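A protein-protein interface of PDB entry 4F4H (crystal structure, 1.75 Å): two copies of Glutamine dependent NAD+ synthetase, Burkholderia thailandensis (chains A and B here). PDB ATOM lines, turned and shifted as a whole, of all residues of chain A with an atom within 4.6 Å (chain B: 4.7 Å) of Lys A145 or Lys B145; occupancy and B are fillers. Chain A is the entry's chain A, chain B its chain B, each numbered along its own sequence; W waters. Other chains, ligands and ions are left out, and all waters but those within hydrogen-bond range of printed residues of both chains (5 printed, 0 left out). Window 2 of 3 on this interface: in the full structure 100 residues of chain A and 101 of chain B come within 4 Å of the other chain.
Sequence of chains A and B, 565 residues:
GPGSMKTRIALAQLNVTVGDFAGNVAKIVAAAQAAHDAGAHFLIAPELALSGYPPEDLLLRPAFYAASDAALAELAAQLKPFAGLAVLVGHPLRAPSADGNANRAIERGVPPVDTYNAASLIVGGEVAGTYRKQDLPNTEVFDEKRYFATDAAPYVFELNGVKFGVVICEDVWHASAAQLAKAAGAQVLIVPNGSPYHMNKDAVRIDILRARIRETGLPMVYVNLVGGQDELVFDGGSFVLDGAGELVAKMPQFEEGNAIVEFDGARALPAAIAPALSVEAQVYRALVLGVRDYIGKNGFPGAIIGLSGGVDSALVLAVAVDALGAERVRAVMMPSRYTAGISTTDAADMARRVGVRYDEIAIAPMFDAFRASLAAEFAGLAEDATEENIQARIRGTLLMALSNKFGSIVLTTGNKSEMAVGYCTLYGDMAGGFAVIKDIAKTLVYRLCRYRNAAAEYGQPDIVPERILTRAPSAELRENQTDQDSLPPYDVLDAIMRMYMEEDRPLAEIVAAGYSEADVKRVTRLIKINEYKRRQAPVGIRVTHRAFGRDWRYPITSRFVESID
The side-chain amide oxygen (OD1) of Asn A138 lies within hydrogen-bond range of the backbone NH (N) of Glu A144. The side-chain amide oxygen (OD1) of Asn A138 lies within hydrogen-bond range of the backbone NH (N) of Lys A145, at 2.9 Å. OD1 of Asn B138 sits at hydrogen-bond distance from N of Glu B144, 3.4 Å away. The backbone NH (N) of Lys B145 lies within hydrogen-bond range of the side-chain amide oxygen (OD1) of Asn B138 (2.9 Å).
Printed residues of chain B within 4 Å of Asn A138: Asn B138 (3.5 Å), Lys B145 (3.8 Å) and Arg B146 (3.5 Å). Lys A145 touches just these residues of chain B: Asn B138 and Lys B145. Of the printed residues of chain B, Arg A146 touches Asn B138 (3.4 Å). Pro B112 touches none of the printed residues of chain A. Of the printed residues of chain A, Asn B138 touches Asn A138, Lys A145 and Arg A146. Printed residues of chain A within 4 Å of Asp B143: Asp A143. Lys B145 touches just these residues of chain A: Asn A138 (3.8 Å) and Lys A145 (3.8 Å). Of the printed residues of chain A, Arg B146 touches Asn A138 (3.5 Å). Phe B148 touches none of the printed residues of chain A. The nearest printed residue of chain B that does not touch Lys A145 is Pro B112 (6.0 Å). The nearest printed residue of chain A that does not touch Lys B145 is Pro A112 (5.9 Å).
Water W5 lies within hydrogen-bond range of the side-chain carboxylate of Asp B143 (2.7 Å), the side-chain carboxylate of Asp A143 (2.8 Å), the side-chain amide nitrogen of Asn B138 (2.9 Å) and the side-chain amide nitrogen of Asn A138 (3.0 Å). Water W1 lies within hydrogen-bond range of NH1 of Arg A146 (2.9 Å), OD1 of Asp B143 (2.9 Å) and O of Asn B138 (3.4 Å). Water W3 lies within hydrogen-bond range of the backbone carbonyl oxygen of Lys A145 (2.9 Å) and the side-chain amino group of Lys B145 (3.1 Å). Water W2 bridges O of Lys B145 (2.9 Å) and NZ of Lys A145 (2.9 Å). Water W4 lies within hydrogen-bond range of OD1 of Asp A143, NH1 of Arg B146 and O of Asn A138.
ND2 of Asn B138 is in hydrogen-bond range of OD1 of Asn A138, at 3.5 Å.
Asn A138 touches its own counterpart, Asn B138. Asn A138 touches Lys B145, and with the chains exchanged Lys A145 touches Asn B138. Asn A138 touches Arg B146, and with the chains exchanged Arg A146 touches Asn B138. Lys A145 touches its own counterpart, Lys B145. 10 positions are printed for both chains.
Of the 10 printed residues of chain A, 4 touch a printed residue of chain B. Among the printed residues, 7 pairs touch across the chains. Among the printed residues, no Asp or Glu carboxylate lies within 4 Å of a Lys or Arg side-chain nitrogen of the other chain.
Among the printed residues, pairs that only touch across the chains: Arg A146 with Asn B138 (3.4 Å), Asn A138 with Arg B146 (3.5 Å), Asp A143 with Asp B143 (3.6 Å), Lys A145 with Lys B145 (3.8 Å), Asn A138 with Lys B145 (3.8 Å) and Lys A145 with Asn B138 (3.9 Å).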
ATOM      1  N   PRO A 112     -26.530  -1.518  -7.472  1.00  0.00           N
ATOM      2  CA  PRO A 112     -27.927  -1.575  -7.937  1.00  0.00           C
ATOM      3  C   PRO A 112     -28.728  -0.469  -7.305  1.00  0.00           C
ATOM      4  O   PRO A 112     -28.498  -0.115  -6.135  1.00  0.00           O
ATOM      5  CB  PRO A 112     -28.414  -2.936  -7.440  1.00  0.00           C
ATOM      6  CG  PRO A 112     -27.192  -3.767  -7.333  1.00  0.00           C
ATOM      7  CD  PRO A 112     -26.032  -2.841  -7.056  1.00  0.00           C
ATOM      8  N   LEU A 136     -30.181  -9.040   1.573  1.00  0.00           N
ATOM      9  CA  LEU A 136     -29.715  -9.709   0.373  1.00  0.00           C
ATOM     10  C   LEU A 136     -28.501 -10.603   0.666  1.00  0.00           C
ATOM     11  O   LEU A 136     -27.519 -10.118   1.135  1.00  0.00           O
ATOM     12  CB  LEU A 136     -29.347  -8.643  -0.661  1.00  0.00           C
ATOM     13  CG  LEU A 136     -30.504  -7.699  -0.992  1.00  0.00           C
ATOM     14  CD1 LEU A 136     -29.967  -6.599  -1.903  1.00  0.00           C
ATOM     15  CD2 LEU A 136     -31.690  -8.428  -1.651  1.00  0.00           C
ATOM     16  N   PRO A 137     -28.591 -11.892   0.351  1.00  0.00           N
ATOM     17  CA  PRO A 137     -27.466 -12.762   0.621  1.00  0.00           C
ATOM     18  C   PRO A 137     -26.307 -12.468  -0.307  1.00  0.00           C
ATOM     19  O   PRO A 137     -26.515 -12.380  -1.526  1.00  0.00           O
ATOM     20  CB  PRO A 137     -28.023 -14.134   0.330  1.00  0.00           C
ATOM     21  CG  PRO A 137     -29.113 -13.930  -0.676  1.00  0.00           C
ATOM     22  CD  PRO A 137     -29.734 -12.625  -0.214  1.00  0.00           C
ATOM     23  N   ASN A 138     -25.095 -12.362   0.252  1.00  0.00           N
ATOM     24  CA  ASN A 138     -23.915 -12.096  -0.578  1.00  0.00           C
ATOM     25  C   ASN A 138     -22.706 -12.783  -0.001  1.00  0.00           C
ATOM     26  O   ASN A 138     -21.669 -12.180   0.245  1.00  0.00           O
ATOM     27  CB  ASN A 138     -23.743 -10.592  -0.704  1.00  0.00           C
ATOM     28  CG  ASN A 138     -23.014 -10.202  -1.949  1.00  0.00           C
ATOM     29  OD1 ASN A 138     -23.618  -9.881  -2.960  1.00  0.00           O
ATOM     30  ND2 ASN A 138     -21.699 -10.227  -1.879  1.00  0.00           N
ATOM     31  N   ASP A 143     -24.878 -13.776  -4.544  1.00  0.00           N
ATOM     32  CA  ASP A 143     -24.245 -12.504  -4.827  1.00  0.00           C
ATOM     33  C   ASP A 143     -25.337 -11.428  -5.060  1.00  0.00           C
ATOM     34  O   ASP A 143     -25.257 -10.636  -6.004  1.00  0.00           O
ATOM     35  CB  ASP A 143     -23.387 -12.628  -6.104  1.00  0.00           C
ATOM     36  CG  ASP A 143     -22.260 -13.612  -5.929  1.00  0.00           C
ATOM     37  OD1 ASP A 143     -21.204 -13.200  -5.420  1.00  0.00           O
ATOM     38  OD2 ASP A 143     -22.435 -14.823  -6.243  1.00  0.00           O
ATOM     39  N   GLU A 144     -26.361 -11.433  -4.247  1.00  0.00           N
ATOM     40  CA  GLU A 144     -27.509 -10.587  -4.548  1.00  0.00           C
ATOM     41  C   GLU A 144     -27.238  -9.075  -4.421  1.00  0.00           C
ATOM     42  O   GLU A 144     -28.019  -8.267  -4.944  1.00  0.00           O
ATOM     43  CB  GLU A 144     -28.778 -11.022  -3.750  1.00  0.00           C
ATOM     44  CG  GLU A 144     -29.347 -12.310  -4.325  1.00  0.00           C
ATOM     45  CD  GLU A 144     -30.787 -12.637  -3.904  1.00  0.00           C
ATOM     46  OE1 GLU A 144     -31.352 -11.940  -3.044  1.00  0.00           O
ATOM     47  OE2 GLU A 144     -31.334 -13.600  -4.486  1.00  0.00           O
ATOM     48  N   LYS A 145     -26.158  -8.685  -3.761  1.00  0.00           N
ATOM     49  CA  LYS A 145     -25.809  -7.254  -3.714  1.00  0.00           C
ATOM     50  C   LYS A 145     -25.154  -6.778  -5.037  1.00  0.00           C
ATOM     51  O   LYS A 145     -25.021  -5.583  -5.266  1.00  0.00           O
ATOM     52  CB  LYS A 145     -24.951  -6.926  -2.515  1.00  0.00           C
ATOM     53  CG  LYS A 145     -25.659  -7.213  -1.186  1.00  0.00           C
ATOM     54  CD  LYS A 145     -24.747  -6.951   0.020  1.00  0.00           C
ATOM     55  CE  LYS A 145     -25.452  -7.320   1.349  1.00  0.00           C
ATOM     56  NZ  LYS A 145     -24.529  -7.111   2.525  1.00  0.00           N
ATOM     57  N   ARG A 146     -24.803  -7.727  -5.915  1.00  0.00           N
ATOM     58  CA  ARG A 146     -24.420  -7.417  -7.301  1.00  0.00           C
ATOM     59  C   ARG A 146     -25.633  -7.049  -8.157  1.00  0.00           C
ATOM     60  O   ARG A 146     -25.499  -6.336  -9.176  1.00  0.00           O
ATOM     61  CB  ARG A 146     -23.717  -8.666  -7.912  1.00  0.00           C
ATOM     62  CG  ARG A 146     -23.093  -8.533  -9.324  1.00  0.00           C
ATOM     63  CD  ARG A 146     -22.627  -9.909  -9.756  1.00  0.00           C
ATOM     64  NE  ARG A 146     -22.130  -9.993 -11.139  1.00  0.00           N
ATOM     65  CZ  ARG A 146     -20.925  -9.620 -11.550  1.00  0.00           C
ATOM     66  NH1 ARG A 146     -20.047  -9.084 -10.719  1.00  0.00           N
ATOM     67  NH2 ARG A 146     -20.602  -9.766 -12.845  1.00  0.00           N
ATOM     68  N   TYR A 147     -26.808  -7.521  -7.749  1.00  0.00           N
ATOM     69  CA  TYR A 147     -28.008  -7.489  -8.587  1.00  0.00           C
ATOM     70  C   TYR A 147     -29.136  -6.597  -8.134  1.00  0.00           C
ATOM     71  O   TYR A 147     -29.857  -6.055  -8.988  1.00  0.00           O
ATOM     72  CB  TYR A 147     -28.563  -8.886  -8.749  1.00  0.00           C
ATOM     73  CG  TYR A 147     -27.576  -9.864  -9.348  1.00  0.00           C
ATOM     74  CD1 TYR A 147     -26.927  -9.581 -10.550  1.00  0.00           C
ATOM     75  CD2 TYR A 147     -27.260 -11.070  -8.700  1.00  0.00           C
ATOM     76  CE1 TYR A 147     -25.977 -10.481 -11.070  1.00  0.00           C
ATOM     77  CE2 TYR A 147     -26.328 -11.975  -9.233  1.00  0.00           C
ATOM     78  CZ  TYR A 147     -25.706 -11.657 -10.443  1.00  0.00           C
ATOM     79  OH  TYR A 147     -24.795 -12.525 -11.031  1.00  0.00           O
ATOM     80  N   PHE A 148     -29.374  -6.551  -6.820  1.00  0.00           N
ATOM     81  CA  PHE A 148     -30.572  -5.975  -6.264  1.00  0.00           C
ATOM     82  C   PHE A 148     -30.251  -4.890  -5.206  1.00  0.00           C
ATOM     83  O   PHE A 148     -29.207  -4.927  -4.526  1.00  0.00           O
ATOM     84  CB  PHE A 148     -31.402  -7.049  -5.551  1.00  0.00           C
ATOM     85  CG  PHE A 148     -31.876  -8.182  -6.423  1.00  0.00           C
ATOM     86  CD1 PHE A 148     -32.629  -7.949  -7.529  1.00  0.00           C
ATOM     87  CD2 PHE A 148     -31.622  -9.495  -6.053  1.00  0.00           C
ATOM     88  CE1 PHE A 148     -33.125  -9.006  -8.300  1.00  0.00           C
ATOM     89  CE2 PHE A 148     -32.097 -10.561  -6.800  1.00  0.00           C
ATOM     90  CZ  PHE A 148     -32.862 -10.303  -7.926  1.00  0.00           C
ATOM     91  N   PRO B 112     -20.104 -10.014   6.488  1.00  0.00           N
ATOM     92  CA  PRO B 112     -18.914  -9.543   7.182  1.00  0.00           C
ATOM     93  C   PRO B 112     -19.290  -8.596   8.319  1.00  0.00           C
ATOM     94  O   PRO B 112     -20.216  -7.770   8.193  1.00  0.00           O
ATOM     95  CB  PRO B 112     -18.145  -8.801   6.081  1.00  0.00           C
ATOM     96  CG  PRO B 112     -18.504  -9.528   4.855  1.00  0.00           C
ATOM     97  CD  PRO B 112     -19.917 -10.002   5.025  1.00  0.00           C
ATOM     98  N   LEU B 136     -17.653  -0.316  -0.765  1.00  0.00           N
ATOM     99  CA  LEU B 136     -17.085  -1.608  -1.164  1.00  0.00           C
ATOM    100  C   LEU B 136     -17.613  -2.026  -2.542  1.00  0.00           C
ATOM    101  O   LEU B 136     -18.816  -2.208  -2.688  1.00  0.00           O
ATOM    102  CB  LEU B 136     -17.446  -2.659  -0.149  1.00  0.00           C
ATOM    103  CG  LEU B 136     -17.023  -2.340   1.278  1.00  0.00           C
ATOM    104  CD1 LEU B 136     -17.553  -3.436   2.223  1.00  0.00           C
ATOM    105  CD2 LEU B 136     -15.515  -2.218   1.382  1.00  0.00           C
ATOM    106  N   PRO B 137     -16.718  -2.172  -3.536  1.00  0.00           N
ATOM    107  CA  PRO B 137     -17.180  -2.530  -4.883  1.00  0.00           C
ATOM    108  C   PRO B 137     -17.700  -3.941  -4.908  1.00  0.00           C
ATOM    109  O   PRO B 137     -16.995  -4.857  -4.451  1.00  0.00           O
ATOM    110  CB  PRO B 137     -15.929  -2.394  -5.741  1.00  0.00           C
ATOM    111  CG  PRO B 137     -14.783  -2.627  -4.796  1.00  0.00           C
ATOM    112  CD  PRO B 137     -15.247  -2.033  -3.486  1.00  0.00           C
ATOM    113  N   ASN B 138     -18.885  -4.123  -5.476  1.00  0.00           N
ATOM    114  CA  ASN B 138     -19.493  -5.450  -5.550  1.00  0.00           C
ATOM    115  C   ASN B 138     -20.238  -5.564  -6.854  1.00  0.00           C
ATOM    116  O   ASN B 138     -21.394  -5.927  -6.907  1.00  0.00           O
ATOM    117  CB  ASN B 138     -20.397  -5.676  -4.336  1.00  0.00           C
ATOM    118  CG  ASN B 138     -20.516  -7.111  -3.998  1.00  0.00           C
ATOM    119  OD1 ASN B 138     -19.743  -7.615  -3.224  1.00  0.00           O
ATOM    120  ND2 ASN B 138     -21.433  -7.817  -4.666  1.00  0.00           N
ATOM    121  N   ASP B 143     -15.971  -8.244  -5.455  1.00  0.00           N
ATOM    122  CA  ASP B 143     -17.008  -8.818  -4.567  1.00  0.00           C
ATOM    123  C   ASP B 143     -16.715  -8.422  -3.127  1.00  0.00           C
ATOM    124  O   ASP B 143     -16.814  -9.248  -2.214  1.00  0.00           O
ATOM    125  CB  ASP B 143     -17.004 -10.335  -4.689  1.00  0.00           C
ATOM    126  CG  ASP B 143     -17.338 -10.790  -6.078  1.00  0.00           C
ATOM    127  OD1 ASP B 143     -18.528 -10.920  -6.360  1.00  0.00           O
ATOM    128  OD2 ASP B 143     -16.441 -10.912  -6.927  1.00  0.00           O
ATOM    129  N   GLU B 144     -16.402  -7.156  -2.897  1.00  0.00           N
ATOM    130  CA  GLU B 144     -15.945  -6.770  -1.562  1.00  0.00           C
ATOM    131  C   GLU B 144     -16.989  -6.857  -0.457  1.00  0.00           C
ATOM    132  O   GLU B 144     -16.626  -6.885   0.742  1.00  0.00           O
ATOM    133  CB  GLU B 144     -15.194  -5.440  -1.575  1.00  0.00           C
ATOM    134  CG  GLU B 144     -13.850  -5.588  -2.275  1.00  0.00           C
ATOM    135  CD  GLU B 144     -12.829  -4.511  -1.969  1.00  0.00           C
ATOM    136  OE1 GLU B 144     -13.197  -3.445  -1.426  1.00  0.00           O
ATOM    137  OE2 GLU B 144     -11.638  -4.777  -2.287  1.00  0.00           O
ATOM    138  N   LYS B 145     -18.269  -6.923  -0.821  1.00  0.00           N
ATOM    139  CA  LYS B 145     -19.306  -7.121   0.204  1.00  0.00           C
ATOM    140  C   LYS B 145     -19.374  -8.581   0.694  1.00  0.00           C
ATOM    141  O   LYS B 145     -20.040  -8.876   1.694  1.00  0.00           O
ATOM    142  CB  LYS B 145     -20.661  -6.597  -0.243  1.00  0.00           C
ATOM    143  CG  LYS B 145     -20.657  -5.083  -0.472  1.00  0.00           C
ATOM    144  CD  LYS B 145     -21.975  -4.564  -1.005  1.00  0.00           C
ATOM    145  CE  LYS B 145     -21.858  -3.084  -1.393  1.00  0.00           C
ATOM    146  NZ  LYS B 145     -23.129  -2.515  -1.883  1.00  0.00           N
ATOM    147  N   ARG B 146     -18.707  -9.480  -0.025  1.00  0.00           N
ATOM    148  CA  ARG B 146     -18.484 -10.859   0.453  1.00  0.00           C
ATOM    149  C   ARG B 146     -17.432 -10.905   1.555  1.00  0.00           C
ATOM    150  O   ARG B 146     -17.450 -11.826   2.381  1.00  0.00           O
ATOM    151  CB  ARG B 146     -18.011 -11.731  -0.733  1.00  0.00           C
ATOM    152  CG  ARG B 146     -17.804 -13.227  -0.487  1.00  0.00           C
ATOM    153  CD  ARG B 146     -17.276 -13.835  -1.781  1.00  0.00           C
ATOM    154  NE  ARG B 146     -16.902 -15.260  -1.677  1.00  0.00           N
ATOM    155  CZ  ARG B 146     -17.738 -16.280  -1.819  1.00  0.00           C
ATOM    156  NH1 ARG B 146     -19.032 -16.094  -2.046  1.00  0.00           N
ATOM    157  NH2 ARG B 146     -17.298 -17.505  -1.708  1.00  0.00           N
ATOM    158  N   TYR B 147     -16.523  -9.918   1.568  1.00  0.00           N
ATOM    159  CA  TYR B 147     -15.303  -9.969   2.398  1.00  0.00           C
ATOM    160  C   TYR B 147     -15.236  -8.966   3.520  1.00  0.00           C
ATOM    161  O   TYR B 147     -14.693  -9.269   4.576  1.00  0.00           O
ATOM    162  CB  TYR B 147     -14.109  -9.774   1.501  1.00  0.00           C
ATOM    163  CG  TYR B 147     -14.019 -10.809   0.406  1.00  0.00           C
ATOM    164  CD1 TYR B 147     -14.133 -12.170   0.704  1.00  0.00           C
ATOM    165  CD2 TYR B 147     -13.862 -10.438  -0.933  1.00  0.00           C
ATOM    166  CE1 TYR B 147     -14.065 -13.135  -0.298  1.00  0.00           C
ATOM    167  CE2 TYR B 147     -13.790 -11.414  -1.960  1.00  0.00           C
ATOM    168  CZ  TYR B 147     -13.882 -12.752  -1.639  1.00  0.00           C
ATOM    169  OH  TYR B 147     -13.780 -13.701  -2.636  1.00  0.00           O
ATOM    170  N   PHE B 148     -15.758  -7.748   3.299  1.00  0.00           N
ATOM    171  CA  PHE B 148     -15.438  -6.642   4.193  1.00  0.00           C
ATOM    172  C   PHE B 148     -16.722  -5.993   4.673  1.00  0.00           C
ATOM    173  O   PHE B 148     -17.767  -6.042   3.982  1.00  0.00           O
ATOM    174  CB  PHE B 148     -14.612  -5.598   3.466  1.00  0.00           C
ATOM    175  CG  PHE B 148     -13.269  -6.067   3.004  1.00  0.00           C
ATOM    176  CD1 PHE B 148     -12.354  -6.560   3.903  1.00  0.00           C
ATOM    177  CD2 PHE B 148     -12.898  -5.937   1.686  1.00  0.00           C
ATOM    178  CE1 PHE B 148     -11.089  -6.954   3.456  1.00  0.00           C
ATOM    179  CE2 PHE B 148     -11.641  -6.309   1.240  1.00  0.00           C
ATOM    180  CZ  PHE B 148     -10.741  -6.824   2.120  1.00  0.00           C
HETATM  181  O   HOH W   1     -19.894  -8.811  -7.878  1.00  0.00           O
HETATM  182  O   HOH W   2     -22.744  -9.404   2.596  1.00  0.00           O
HETATM  183  O   HOH W   3     -23.239  -3.382  -4.819  1.00  0.00           O
HETATM  184  O   HOH W   4     -20.646 -13.703  -2.589  1.00  0.00           O
HETATM  185  O   HOH W   5     -20.579 -10.638  -4.637  1.00  0.00           O
